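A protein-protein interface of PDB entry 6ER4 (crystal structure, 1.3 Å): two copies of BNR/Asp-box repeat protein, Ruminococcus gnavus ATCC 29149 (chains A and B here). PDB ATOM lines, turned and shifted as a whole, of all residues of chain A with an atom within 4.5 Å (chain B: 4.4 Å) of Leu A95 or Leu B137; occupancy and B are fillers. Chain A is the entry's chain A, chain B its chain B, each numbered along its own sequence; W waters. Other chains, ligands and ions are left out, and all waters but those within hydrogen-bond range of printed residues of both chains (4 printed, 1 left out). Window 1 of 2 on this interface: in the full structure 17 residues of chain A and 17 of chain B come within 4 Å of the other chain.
N of Gln B139 sits at hydrogen-bond distance from O of Lys B123, 3.1 Å away.
N of Leu A127 sits at hydrogen-bond distance from O of Ala A135, 3.0 Å away.
N of Cys A97 is in hydrogen-bond range of O of Val A80 (2.8 Å).
N of Tyr B125 lies within hydrogen-bond range of O of Leu B137, 2.8 Å away.
The backbone NH (N) of Leu A95 is in hydrogen-bond range of the backbone carbonyl oxygen (O) of Met A82 (3.0 Å).
OE1 of Gln B124 lies close to OD1 of Asp B138, 3.5 Å away.
Printed residues of chain A that touch a printed residue of chain B: Thr A94, Leu A95, Asp A96, Cys A97, Ala A135, Thr A136 and Leu A137.
Of the 10 printed residues of chain B, 7 touch a printed residue of chain A.
Printed residues of chain B that touch a printed residue of chain A: Tyr B93, Thr B94, Leu B95, Thr B136, Leu B137, Asp B138 and Gln B139.
Among the printed residues, 11 pairs touch across the chains.
Among the printed residues, no Asp or Glu carboxylate lies within 4 Å of a Lys or Arg side-chain nitrogen of the other chain.
Thr A94 touches its own counterpart, Thr B94.
Leu A95 touches Leu B137, and with the chains exchanged Leu A137 touches Leu B95.
Thr B136 touches its own counterpart, Thr A136.
Thr A136 touches Leu B137, and with the chains exchanged Leu A137 touches Thr B136.
Positions printed for both chains: 94, 95, 136 and 137.
Of the 11 pairs that touch across the chains among the printed residues, 6 have their exchanged pair printed and touching as well.
The side-chain amide nitrogen (NE2) of Gln B139 lies within hydrogen-bond range of the side-chain sulfur (SG) of Cys A97.
The side-chain hydroxyl (OG1) of Thr B94 lies within hydrogen-bond range of the side-chain hydroxyl (OG1) of Thr A94, at 3.1 Å.
The backbone NH of Asp B138 sits at hydrogen-bond distance from the backbone carbonyl oxygen of Thr A136 (2.8 Å).
Water W3 bridges the side-chain amide oxygen of Gln B139 and the backbone carbonyl oxygen of Asp A96.
Water W4 bridges OG1 of Thr A94 (2.8 Å) and OG1 of Thr B94 (2.8 Å).
Water W2 bridges the side-chain hydroxyl (OG1) of Thr A136 and the backbone carbonyl oxygen (O) of Asp B138.
Water W1 bridges the backbone NH (N) of Thr B94 (3.0 Å) and the backbone carbonyl oxygen (O) of Thr A94 (3.5 Å).
Among the printed residues, merely in contact across the chains: Leu A95 with Leu B137 (3.5 Å), Asp A96 with Tyr B93 (3.5 Å), Ala A135 with Asp B138 (3.2 Å), Ala A135 with Gln B139 (3.9 Å), Thr A136 with Thr B136 (3.9 Å), Thr A136 with Leu B137 (3.4 Å), Leu A137 with Leu B95 (3.5 Å) and Leu A137 with Thr B136 (3.4 Å).
Tyr A73 touches none of the printed residues of chain B.
Val A80 touches none of the printed residues of chain B.
Printed residues of chain B within 4 Å of Thr A94: Thr B94 (3.1 Å).
Leu A95 touches one residue of chain B.
Of the printed residues of chain A, Thr B136 touches Thr A136 (3.9 Å) and Leu A137 (3.4 Å).
Of chain A, only Leu A95 (3.5 Å) and Thr A136 (3.4 Å) come within 4 Å of Leu B137.
The nearest printed residue of chain B that does not touch Asp A96 is Gln B139 (4.02 Å).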
ATOM      1  N   TYR A  73      10.229  14.702  -7.938  1.00  0.00           N
ATOM      2  CA  TYR A  73       9.625  13.653  -8.769  1.00  0.00           C
ATOM      3  C   TYR A  73       8.400  14.158  -9.521  1.00  0.00           C
ATOM      4  O   TYR A  73       7.807  15.168  -9.165  1.00  0.00           O
ATOM      5  CB  TYR A  73       9.271  12.419  -7.941  1.00  0.00           C
ATOM      6  CG  TYR A  73       8.150  12.592  -6.964  1.00  0.00           C
ATOM      7  CD1 TYR A  73       6.821  12.422  -7.353  1.00  0.00           C
ATOM      8  CD2 TYR A  73       8.390  12.953  -5.640  1.00  0.00           C
ATOM      9  CE1 TYR A  73       5.784  12.562  -6.466  1.00  0.00           C
ATOM     10  CE2 TYR A  73       7.343  13.085  -4.754  1.00  0.00           C
ATOM     11  CZ  TYR A  73       6.052  12.897  -5.159  1.00  0.00           C
ATOM     12  OH  TYR A  73       5.040  13.035  -4.254  1.00  0.00           O
ATOM     13  N   VAL A  80       3.466  16.647  -9.662  1.00  0.00           N
ATOM     14  CA  VAL A  80       4.852  17.010  -9.311  1.00  0.00           C
ATOM     15  C   VAL A  80       4.929  16.990  -7.802  1.00  0.00           C
ATOM     16  O   VAL A  80       4.021  17.472  -7.131  1.00  0.00           O
ATOM     17  CB  VAL A  80       5.232  18.401  -9.861  1.00  0.00           C
ATOM     18  CG1 VAL A  80       6.691  18.758  -9.551  1.00  0.00           C
ATOM     19  CG2 VAL A  80       4.998  18.528 -11.339  1.00  0.00           C
ATOM     20  N   GLY A  81       6.040  16.466  -7.285  1.00  0.00           N
ATOM     21  CA  GLY A  81       6.242  16.476  -5.853  1.00  0.00           C
ATOM     22  C   GLY A  81       7.677  16.438  -5.431  1.00  0.00           C
ATOM     23  O   GLY A  81       8.577  16.342  -6.242  1.00  0.00           O
ATOM     24  N   MET A  82       7.876  16.469  -4.111  1.00  0.00           N
ATOM     25  CA  MET A  82       9.196  16.219  -3.525  1.00  0.00           C
ATOM     26  C   MET A  82       9.022  15.502  -2.217  1.00  0.00           C
ATOM     27  O   MET A  82       7.964  15.600  -1.572  1.00  0.00           O
ATOM     28  CB  MET A  82       9.986  17.500  -3.369  1.00  0.00           C
ATOM     29  CG  MET A  82       9.518  18.404  -2.273  1.00  0.00           C
ATOM     30  SD  MET A  82      10.400  18.056  -0.736  1.00  0.00           S
ATOM     31  CE  MET A  82       9.533  19.171   0.382  1.00  0.00           C
ATOM     32  N   THR A  94       7.071  16.692   2.651  1.00  0.00           N
ATOM     33  CA  THR A  94       6.662  16.336   1.304  1.00  0.00           C
ATOM     34  C   THR A  94       5.733  17.365   0.704  1.00  0.00           C
ATOM     35  O   THR A  94       5.041  18.114   1.402  1.00  0.00           O
ATOM     36  CB  THR A  94       5.929  14.971   1.299  1.00  0.00           C
ATOM     37  OG1 THR A  94       4.661  15.120   1.885  1.00  0.00           O
ATOM     38  CG2 THR A  94       6.692  13.893   1.988  1.00  0.00           C
ATOM     39  N   LEU A  95       5.771  17.390  -0.617  1.00  0.00           N
ATOM     40  CA  LEU A  95       4.786  18.090  -1.436  1.00  0.00           C
ATOM     41  C   LEU A  95       4.311  17.144  -2.540  1.00  0.00           C
ATOM     42  O   LEU A  95       5.054  16.326  -3.029  1.00  0.00           O
ATOM     43  CB  LEU A  95       5.358  19.355  -2.078  1.00  0.00           C
ATOM     44  CG  LEU A  95       5.684  20.511  -1.123  1.00  0.00           C
ATOM     45  CD1 LEU A  95       6.419  21.665  -1.785  1.00  0.00           C
ATOM     46  CD2 LEU A  95       4.360  21.077  -0.533  1.00  0.00           C
ATOM     47  N   ASP A  96       3.061  17.315  -2.937  1.00  0.00           N
ATOM     48  CA  ASP A  96       2.475  16.573  -4.043  1.00  0.00           C
ATOM     49  C   ASP A  96       1.372  17.426  -4.633  1.00  0.00           C
ATOM     50  O   ASP A  96       0.412  17.772  -3.923  1.00  0.00           O
ATOM     51  CB  ASP A  96       1.949  15.222  -3.570  1.00  0.00           C
ATOM     52  CG  ASP A  96       1.833  14.284  -4.665  1.00  0.00           C
ATOM     53  OD1 ASP A  96       0.792  14.371  -5.330  1.00  0.00           O
ATOM     54  OD2 ASP A  96       2.797  13.525  -4.930  1.00  0.00           O
ATOM     55  N   CYS A  97       1.539  17.815  -5.896  1.00  0.00           N
ATOM     56  CA  CYS A  97       0.647  18.783  -6.557  1.00  0.00           C
ATOM     57  C   CYS A  97       0.050  18.138  -7.761  1.00  0.00           C
ATOM     58  O   CYS A  97       0.797  17.686  -8.660  1.00  0.00           O
ATOM     59  CB  CYS A  97       1.408  20.017  -7.008  1.00  0.00           C
ATOM     60  SG  CYS A  97       2.200  20.854  -5.643  1.00  0.00           S
ATOM     61  N   LEU A 127       7.569  24.959  -4.810  1.00  0.00           N
ATOM     62  CA  LEU A 127       7.556  24.091  -5.970  1.00  0.00           C
ATOM     63  C   LEU A 127       6.913  24.832  -7.138  1.00  0.00           C
ATOM     64  O   LEU A 127       5.859  25.475  -6.983  1.00  0.00           O
ATOM     65  CB  LEU A 127       6.747  22.851  -5.619  1.00  0.00           C
ATOM     66  CG  LEU A 127       6.808  21.690  -6.559  1.00  0.00           C
ATOM     67  CD1 LEU A 127       8.235  21.124  -6.753  1.00  0.00           C
ATOM     68  CD2 LEU A 127       5.920  20.584  -6.028  1.00  0.00           C
ATOM     69  N   ALA A 135       3.019  25.187  -5.073  1.00  0.00           N
ATOM     70  CA  ALA A 135       2.884  24.919  -3.635  1.00  0.00           C
ATOM     71  C   ALA A 135       3.987  25.590  -2.875  1.00  0.00           C
ATOM     72  O   ALA A 135       5.084  25.752  -3.400  1.00  0.00           O
ATOM     73  CB  ALA A 135       2.884  23.425  -3.317  1.00  0.00           C
ATOM     74  N   THR A 136       3.674  25.920  -1.617  1.00  0.00           N
ATOM     75  CA  THR A 136       4.598  26.491  -0.675  1.00  0.00           C
ATOM     76  C   THR A 136       4.455  25.745   0.642  1.00  0.00           C
ATOM     77  O   THR A 136       3.335  25.482   1.082  1.00  0.00           O
ATOM     78  CB  THR A 136       4.274  27.995  -0.429  1.00  0.00           C
ATOM     79  OG1 THR A 136       4.272  28.700  -1.671  1.00  0.00           O
ATOM     80  CG2 THR A 136       5.262  28.642   0.499  1.00  0.00           C
ATOM     81  N   LEU A 137       5.578  25.402   1.267  1.00  0.00           N
ATOM     82  CA  LEU A 137       5.577  24.706   2.565  1.00  0.00           C
ATOM     83  C   LEU A 137       6.529  25.417   3.514  1.00  0.00           C
ATOM     84  O   LEU A 137       7.680  25.610   3.176  1.00  0.00           O
ATOM     85  CB  LEU A 137       6.050  23.232   2.358  1.00  0.00           C
ATOM     86  CG  LEU A 137       6.213  22.387   3.632  1.00  0.00           C
ATOM     87  CD1 LEU A 137       4.872  22.155   4.310  1.00  0.00           C
ATOM     88  CD2 LEU A 137       6.848  21.050   3.316  1.00  0.00           C
ATOM     89  N   TYR B  93      -2.676  15.891  -0.025  1.00  0.00           N
ATOM     90  CA  TYR B  93      -2.047  17.039   0.647  1.00  0.00           C
ATOM     91  C   TYR B  93      -1.794  16.670   2.094  1.00  0.00           C
ATOM     92  O   TYR B  93      -2.716  16.243   2.806  1.00  0.00           O
ATOM     93  CB  TYR B  93      -2.961  18.248   0.610  1.00  0.00           C
ATOM     94  CG  TYR B  93      -3.267  18.791  -0.762  1.00  0.00           C
ATOM     95  CD1 TYR B  93      -2.517  18.433  -1.900  1.00  0.00           C
ATOM     96  CD2 TYR B  93      -4.298  19.676  -0.943  1.00  0.00           C
ATOM     97  CE1 TYR B  93      -2.813  18.979  -3.139  1.00  0.00           C
ATOM     98  CE2 TYR B  93      -4.601  20.218  -2.182  1.00  0.00           C
ATOM     99  CZ  TYR B  93      -3.835  19.867  -3.292  1.00  0.00           C
ATOM    100  OH  TYR B  93      -4.112  20.380  -4.541  1.00  0.00           O
ATOM    101  N   THR B  94      -0.550  16.764   2.523  1.00  0.00           N
ATOM    102  CA  THR B  94      -0.138  16.296   3.818  1.00  0.00           C
ATOM    103  C   THR B  94       0.759  17.275   4.553  1.00  0.00           C
ATOM    104  O   THR B  94       1.486  18.067   3.941  1.00  0.00           O
ATOM    105  CB  THR B  94       0.572  14.935   3.711  1.00  0.00           C
ATOM    106  OG1 THR B  94       1.843  15.124   3.129  1.00  0.00           O
ATOM    107  CG2 THR B  94      -0.203  13.908   2.924  1.00  0.00           C
ATOM    108  N   LEU B  95       0.730  17.153   5.876  1.00  0.00           N
ATOM    109  CA  LEU B  95       1.751  17.722   6.748  1.00  0.00           C
ATOM    110  C   LEU B  95       2.230  16.655   7.730  1.00  0.00           C
ATOM    111  O   LEU B  95       1.459  15.788   8.146  1.00  0.00           O
ATOM    112  CB  LEU B  95       1.206  18.912   7.505  1.00  0.00           C
ATOM    113  CG  LEU B  95       0.915  20.158   6.663  1.00  0.00           C
ATOM    114  CD1 LEU B  95       0.184  21.223   7.461  1.00  0.00           C
ATOM    115  CD2 LEU B  95       2.254  20.749   6.127  1.00  0.00           C
ATOM    116  N   LYS B 123      -5.943  29.831   0.439  1.00  0.00           N
ATOM    117  CA  LYS B 123      -5.507  28.525  -0.087  1.00  0.00           C
ATOM    118  C   LYS B 123      -4.425  27.924   0.807  1.00  0.00           C
ATOM    119  O   LYS B 123      -3.437  27.411   0.335  1.00  0.00           O
ATOM    120  CB  LYS B 123      -5.079  28.594  -1.556  1.00  0.00           C
ATOM    121  CG  LYS B 123      -6.212  29.054  -2.469  1.00  0.00           C
ATOM    122  CD  LYS B 123      -6.055  28.752  -3.948  1.00  0.00           C
ATOM    123  CE  LYS B 123      -5.079  29.702  -4.555  1.00  0.00           C
ATOM    124  NZ  LYS B 123      -4.859  29.424  -5.983  1.00  0.00           N
ATOM    125  N   GLN B 124      -4.676  27.932   2.102  1.00  0.00           N
ATOM    126  CA  GLN B 124      -3.643  27.693   3.110  1.00  0.00           C
ATOM    127  C   GLN B 124      -4.127  26.738   4.183  1.00  0.00           C
ATOM    128  O   GLN B 124      -5.278  26.811   4.602  1.00  0.00           O
ATOM    129  CB  GLN B 124      -3.336  29.081   3.725  1.00  0.00           C
ATOM    130  CG  GLN B 124      -2.264  29.149   4.705  1.00  0.00           C
ATOM    131  CD  GLN B 124      -2.132  30.641   5.112  1.00  0.00           C
ATOM    132  OE1 GLN B 124      -1.225  31.325   4.694  1.00  0.00           O
ATOM    133  NE2 GLN B 124      -3.141  31.152   5.829  1.00  0.00           N
ATOM    134  N   TYR B 125      -3.233  25.866   4.639  1.00  0.00           N
ATOM    135  CA  TYR B 125      -3.438  25.010   5.806  1.00  0.00           C
ATOM    136  C   TYR B 125      -2.388  25.368   6.807  1.00  0.00           C
ATOM    137  O   TYR B 125      -1.217  25.509   6.440  1.00  0.00           O
ATOM    138  CB  TYR B 125      -3.292  23.524   5.415  1.00  0.00           C
ATOM    139  CG  TYR B 125      -4.047  23.127   4.166  1.00  0.00           C
ATOM    140  CD1 TYR B 125      -3.445  23.222   2.925  1.00  0.00           C
ATOM    141  CD2 TYR B 125      -5.337  22.662   4.212  1.00  0.00           C
ATOM    142  CE1 TYR B 125      -4.129  22.905   1.778  1.00  0.00           C
ATOM    143  CE2 TYR B 125      -6.046  22.353   3.058  1.00  0.00           C
ATOM    144  CZ  TYR B 125      -5.412  22.421   1.836  1.00  0.00           C
ATOM    145  OH  TYR B 125      -6.093  22.099   0.676  1.00  0.00           O
ATOM    146  N   THR B 136       2.986  25.360   7.718  1.00  0.00           N
ATOM    147  CA  THR B 136       2.008  25.986   6.822  1.00  0.00           C
ATOM    148  C   THR B 136       2.165  25.358   5.450  1.00  0.00           C
ATOM    149  O   THR B 136       3.297  25.210   4.977  1.00  0.00           O
ATOM    150  CB  THR B 136       2.256  27.506   6.703  1.00  0.00           C
ATOM    151  OG1 THR B 136       2.129  28.093   8.004  1.00  0.00           O
ATOM    152  CG2 THR B 136       1.306  28.203   5.760  1.00  0.00           C
ATOM    153  N   LEU B 137       1.049  25.069   4.786  1.00  0.00           N
ATOM    154  CA  LEU B 137       1.049  24.564   3.415  1.00  0.00           C
ATOM    155  C   LEU B 137       0.122  25.434   2.601  1.00  0.00           C
ATOM    156  O   LEU B 137      -1.045  25.645   2.967  1.00  0.00           O
ATOM    157  CB  LEU B 137       0.554  23.123   3.409  1.00  0.00           C
ATOM    158  CG  LEU B 137       0.383  22.446   2.021  1.00  0.00           C
ATOM    159  CD1 LEU B 137       1.723  22.297   1.350  1.00  0.00           C
ATOM    160  CD2 LEU B 137      -0.276  21.087   2.204  1.00  0.00           C
ATOM    161  N   ASP B 138       0.614  25.940   1.460  1.00  0.00           N
ATOM    162  CA  ASP B 138      -0.209  26.710   0.521  1.00  0.00           C
ATOM    163  C   ASP B 138      -0.259  25.911  -0.769  1.00  0.00           C
ATOM    164  O   ASP B 138       0.794  25.571  -1.300  1.00  0.00           O
ATOM    165  CB  ASP B 138       0.417  28.100   0.238  1.00  0.00           C
ATOM    166  CG  ASP B 138       0.726  28.912   1.466  1.00  0.00           C
ATOM    167  OD1 ASP B 138      -0.147  29.121   2.263  1.00  0.00           O
ATOM    168  OD2 ASP B 138       1.852  29.408   1.622  1.00  0.00           O
ATOM    169  N   GLN B 139      -1.449  25.613  -1.294  1.00  0.00           N
ATOM    170  CA  GLN B 139      -1.609  24.807  -2.529  1.00  0.00           C
ATOM    171  C   GLN B 139      -2.335  25.615  -3.542  1.00  0.00           C
ATOM    172  O   GLN B 139      -3.433  26.124  -3.244  1.00  0.00           O
ATOM    173  CB  GLN B 139      -2.460  23.552  -2.286  1.00  0.00           C
ATOM    174  CG  GLN B 139      -1.770  22.531  -1.470  1.00  0.00           C
ATOM    175  CD  GLN B 139      -0.643  21.775  -2.102  1.00  0.00           C
ATOM    176  OE1 GLN B 139       0.176  21.277  -1.341  1.00  0.00           O
ATOM    177  NE2 GLN B 139      -0.559  21.649  -3.464  1.00  0.00           N
HETATM  178  O   HOH W   1       1.735  17.214   0.710  1.00  0.00           O
HETATM  179  O   HOH W   2       1.916  28.111  -3.143  1.00  0.00           O
HETATM  180  O   HOH W   3       1.052  18.838  -1.445  1.00  0.00           O
HETATM  181  O   HOH W   4       3.231  12.807   2.332  1.00  0.00           O
